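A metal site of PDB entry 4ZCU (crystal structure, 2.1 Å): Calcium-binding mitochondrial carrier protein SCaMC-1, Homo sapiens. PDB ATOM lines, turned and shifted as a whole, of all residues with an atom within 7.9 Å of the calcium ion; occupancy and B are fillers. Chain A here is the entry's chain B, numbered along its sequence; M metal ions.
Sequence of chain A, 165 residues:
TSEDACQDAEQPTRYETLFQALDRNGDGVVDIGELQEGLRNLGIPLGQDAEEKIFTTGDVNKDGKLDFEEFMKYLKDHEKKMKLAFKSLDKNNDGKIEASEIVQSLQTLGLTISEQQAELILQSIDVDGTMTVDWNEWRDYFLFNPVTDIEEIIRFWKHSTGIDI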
ATOM      1  N   PHE A  86     -28.484 -12.576  21.080  1.00  0.00           N
ATOM      2  CA  PHE A  86     -27.246 -11.814  20.943  1.00  0.00           C
ATOM      3  C   PHE A  86     -27.495 -10.325  21.095  1.00  0.00           C
ATOM      4  O   PHE A  86     -26.866  -9.663  21.912  1.00  0.00           O
ATOM      5  CB  PHE A  86     -26.591 -12.097  19.593  1.00  0.00           C
ATOM      6  CG  PHE A  86     -25.238 -11.447  19.428  1.00  0.00           C
ATOM      7  CD1 PHE A  86     -25.114 -10.178  18.882  1.00  0.00           C
ATOM      8  CD2 PHE A  86     -24.081 -12.105  19.834  1.00  0.00           C
ATOM      9  CE1 PHE A  86     -23.877  -9.590  18.742  1.00  0.00           C
ATOM     10  CE2 PHE A  86     -22.844 -11.516  19.694  1.00  0.00           C
ATOM     11  CZ  PHE A  86     -22.742 -10.259  19.148  1.00  0.00           C
ATOM     12  N   LEU A  89     -28.327  -9.201  24.474  1.00  0.00           N
ATOM     13  CA  LEU A  89     -27.168  -9.154  25.375  1.00  0.00           C
ATOM     14  C   LEU A  89     -26.284  -7.940  25.104  1.00  0.00           C
ATOM     15  O   LEU A  89     -25.722  -7.359  26.026  1.00  0.00           O
ATOM     16  CB  LEU A  89     -26.335 -10.436  25.245  1.00  0.00           C
ATOM     17  CG  LEU A  89     -26.957 -11.727  25.764  1.00  0.00           C
ATOM     18  CD1 LEU A  89     -25.932 -12.841  25.768  1.00  0.00           C
ATOM     19  CD2 LEU A  89     -27.564 -11.543  27.135  1.00  0.00           C
ATOM     20  N   ASP A  90     -26.153  -7.570  23.832  1.00  0.00           N
ATOM     21  CA  ASP A  90     -25.295  -6.466  23.442  1.00  0.00           C
ATOM     22  C   ASP A  90     -25.959  -5.136  23.757  1.00  0.00           C
ATOM     23  O   ASP A  90     -26.676  -4.570  22.928  1.00  0.00           O
ATOM     24  CB  ASP A  90     -24.937  -6.558  21.958  1.00  0.00           C
ATOM     25  CG  ASP A  90     -23.808  -5.613  21.577  1.00  0.00           C
ATOM     26  OD1 ASP A  90     -23.134  -5.084  22.495  1.00  0.00           O
ATOM     27  OD2 ASP A  90     -23.590  -5.405  20.370  1.00  0.00           O
ATOM     28  N   LYS A  91     -25.698  -4.638  24.958  1.00  0.00           N
ATOM     29  CA  LYS A  91     -26.335  -3.434  25.478  1.00  0.00           C
ATOM     30  C   LYS A  91     -25.819  -2.161  24.810  1.00  0.00           C
ATOM     31  O   LYS A  91     -26.592  -1.227  24.550  1.00  0.00           O
ATOM     32  CB  LYS A  91     -26.160  -3.325  27.002  1.00  0.00           C
ATOM     33  CG  LYS A  91     -26.684  -4.529  27.791  1.00  0.00           C
ATOM     34  CD  LYS A  91     -28.198  -4.634  27.695  1.00  0.00           C
ATOM     35  CE  LYS A  91     -28.739  -5.735  28.607  1.00  0.00           C
ATOM     36  NZ  LYS A  91     -30.070  -6.214  28.149  1.00  0.00           N
ATOM     37  N   ASN A  92     -24.525  -2.116  24.518  1.00  0.00           N
ATOM     38  CA  ASN A  92     -23.907  -0.924  23.948  1.00  0.00           C
ATOM     39  C   ASN A  92     -23.818  -0.996  22.418  1.00  0.00           C
ATOM     40  O   ASN A  92     -23.205  -0.141  21.785  1.00  0.00           O
ATOM     41  CB  ASN A  92     -22.519  -0.692  24.546  1.00  0.00           C
ATOM     42  CG  ASN A  92     -21.526  -1.764  24.134  1.00  0.00           C
ATOM     43  OD1 ASN A  92     -21.904  -2.864  23.755  1.00  0.00           O
ATOM     44  ND2 ASN A  92     -20.241  -1.434  24.218  1.00  0.00           N
ATOM     45  N   ASN A  93     -24.422  -2.038  21.854  1.00  0.00           N
ATOM     46  CA  ASN A  93     -24.516  -2.222  20.410  1.00  0.00           C
ATOM     47  C   ASN A  93     -23.189  -2.134  19.672  1.00  0.00           C
ATOM     48  O   ASN A  93     -23.133  -1.637  18.553  1.00  0.00           O
ATOM     49  CB  ASN A  93     -25.484  -1.193  19.810  1.00  0.00           C
ATOM     50  CG  ASN A  93     -26.916  -1.391  20.277  1.00  0.00           C
ATOM     51  OD1 ASN A  93     -27.330  -2.506  20.591  1.00  0.00           O
ATOM     52  ND2 ASN A  93     -27.671  -0.310  20.324  1.00  0.00           N
ATOM     53  N   ASP A  94     -22.119  -2.649  20.286  1.00  0.00           N
ATOM     54  CA  ASP A  94     -20.816  -2.637  19.627  1.00  0.00           C
ATOM     55  C   ASP A  94     -20.586  -3.909  18.802  1.00  0.00           C
ATOM     56  O   ASP A  94     -19.491  -4.135  18.294  1.00  0.00           O
ATOM     57  CB  ASP A  94     -19.695  -2.433  20.660  1.00  0.00           C
ATOM     58  CG  ASP A  94     -19.668  -3.490  21.747  1.00  0.00           C
ATOM     59  OD1 ASP A  94     -20.371  -4.514  21.617  1.00  0.00           O
ATOM     60  OD2 ASP A  94     -18.920  -3.297  22.732  1.00  0.00           O
ATOM     61  N   GLY A  95     -21.648  -4.723  18.672  1.00  0.00           N
ATOM     62  CA  GLY A  95     -21.631  -5.954  17.887  1.00  0.00           C
ATOM     63  C   GLY A  95     -20.820  -7.018  18.592  1.00  0.00           C
ATOM     64  O   GLY A  95     -20.370  -8.008  18.007  1.00  0.00           O
ATOM     65  N   LYS A  96     -20.586  -6.789  19.877  1.00  0.00           N
ATOM     66  CA  LYS A  96     -19.754  -7.686  20.648  1.00  0.00           C
ATOM     67  C   LYS A  96     -20.327  -7.886  22.071  1.00  0.00           C
ATOM     68  O   LYS A  96     -21.163  -7.095  22.515  1.00  0.00           O
ATOM     69  CB  LYS A  96     -18.368  -7.060  20.604  1.00  0.00           C
ATOM     70  CG  LYS A  96     -17.221  -7.857  21.097  1.00  0.00           C
ATOM     71  CD  LYS A  96     -15.926  -7.104  20.790  1.00  0.00           C
ATOM     72  CE  LYS A  96     -14.896  -7.480  21.786  1.00  0.00           C
ATOM     73  NZ  LYS A  96     -15.479  -7.251  23.167  1.00  0.00           N
ATOM     74  N   ILE A  97     -19.906  -8.935  22.769  1.00  0.00           N
ATOM     75  CA  ILE A  97     -20.445  -9.171  24.106  1.00  0.00           C
ATOM     76  C   ILE A  97     -19.375  -9.170  25.185  1.00  0.00           C
ATOM     77  O   ILE A  97     -18.501 -10.043  25.214  1.00  0.00           O
ATOM     78  CB  ILE A  97     -21.221 -10.504  24.167  1.00  0.00           C
ATOM     79  CG1 ILE A  97     -22.442 -10.454  23.249  1.00  0.00           C
ATOM     80  CG2 ILE A  97     -21.658 -10.821  25.603  1.00  0.00           C
ATOM     81  CD1 ILE A  97     -23.260 -11.727  23.234  1.00  0.00           C
ATOM     82  N   GLU A  98     -19.453  -8.186  26.068  1.00  0.00           N
ATOM     83  CA  GLU A  98     -18.542  -8.078  27.201  1.00  0.00           C
ATOM     84  C   GLU A  98     -19.137  -8.759  28.419  1.00  0.00           C
ATOM     85  O   GLU A  98     -20.343  -8.994  28.476  1.00  0.00           O
ATOM     86  CB  GLU A  98     -18.214  -6.616  27.496  1.00  0.00           C
ATOM     87  CG  GLU A  98     -17.355  -5.930  26.428  1.00  0.00           C
ATOM     88  CD  GLU A  98     -18.171  -5.466  25.235  1.00  0.00           C
ATOM     89  OE1 GLU A  98     -19.408  -5.364  25.355  1.00  0.00           O
ATOM     90  OE2 GLU A  98     -17.573  -5.192  24.175  1.00  0.00           O
ATOM     91  N   ALA A  99     -18.286  -9.085  29.396  1.00  0.00           N
ATOM     92  CA  ALA A  99     -18.730  -9.802  30.593  1.00  0.00           C
ATOM     93  C   ALA A  99     -19.748  -8.998  31.397  1.00  0.00           C
ATOM     94  O   ALA A  99     -20.701  -9.558  31.939  1.00  0.00           O
ATOM     95  CB  ALA A  99     -17.534 -10.149  31.461  1.00  0.00           C
ATOM     96  N   SER A 100     -19.533  -7.686  31.461  1.00  0.00           N
ATOM     97  CA  SER A 100     -20.429  -6.795  32.175  1.00  0.00           C
ATOM     98  C   SER A 100     -21.850  -6.849  31.611  1.00  0.00           C
ATOM     99  O   SER A 100     -22.822  -6.726  32.352  1.00  0.00           O
ATOM    100  CB  SER A 100     -19.902  -5.356  32.141  1.00  0.00           C
ATOM    101  OG  SER A 100     -19.714  -4.917  30.803  1.00  0.00           O
ATOM    102  N   GLU A 101     -21.954  -7.045  30.296  1.00  0.00           N
ATOM    103  CA  GLU A 101     -23.254  -7.140  29.644  1.00  0.00           C
ATOM    104  C   GLU A 101     -23.980  -8.429  30.050  1.00  0.00           C
ATOM    105  O   GLU A 101     -25.191  -8.437  30.236  1.00  0.00           O
ATOM    106  CB  GLU A 101     -23.086  -7.068  28.126  1.00  0.00           C
ATOM    107  CG  GLU A 101     -22.646  -5.685  27.629  1.00  0.00           C
ATOM    108  CD  GLU A 101     -22.411  -5.612  26.134  1.00  0.00           C
ATOM    109  OE1 GLU A 101     -21.986  -6.633  25.535  1.00  0.00           O
ATOM    110  OE2 GLU A 101     -22.655  -4.537  25.550  1.00  0.00           O
ATOM    111  N   VAL A 133     -16.675 -11.934  23.030  1.00  0.00           N
ATOM    112  CA  VAL A 133     -17.243 -12.662  21.885  1.00  0.00           C
ATOM    113  C   VAL A 133     -18.077 -11.798  20.917  1.00  0.00           C
ATOM    114  O   VAL A 133     -18.908 -11.001  21.357  1.00  0.00           O
ATOM    115  CB  VAL A 133     -18.129 -13.833  22.386  1.00  0.00           C
ATOM    116  CG1 VAL A 133     -18.882 -14.471  21.233  1.00  0.00           C
ATOM    117  CG2 VAL A 133     -17.279 -14.865  23.101  1.00  0.00           C
HETATM  118 CA    CA M   1     -21.185  -5.135  23.800  1.00  0.00          CA
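Six residues have an atom within 4 Å of the calcium ion: Asp 90, Asn 92, Asp 94, Lys 96, Glu 98 and Glu 101. The nearest printed residue that does not touch the calcium ion is Ile 97 (4.1 Å).
The calcium ion is bound by the backbone carbonyl oxygen (O) of Lys 96 (2.3 Å), the side-chain carboxylate (OD1) of Asp 90 (2.3 Å), the side-chain carboxylate (OE2) of Glu 101 (2.4 Å), the side-chain carboxylate (OE1) of Glu 98 (2.4 Å), the side-chain amide oxygen (OD1) of Asn 92 (2.4 Å), the side-chain carboxylate (OD1) of Asp 94 (2.4 Å) and the side-chain carboxylate (OE1) of Glu 101 (2.4 Å). The calcium ion has seven donor atoms within binding distance. Slightly farther from the calcium ion lies the side-chain carboxylate (OD2) of Asp 94 (3.1 Å).
O of Asp 90 lies close to OD1 of Asn 93 (3.2 Å). OD2 of Asp 90 sits at hydrogen-bond distance from N of Gly 95 (2.7 Å). OE2 of Glu 101 sits close to N of Lys 91.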
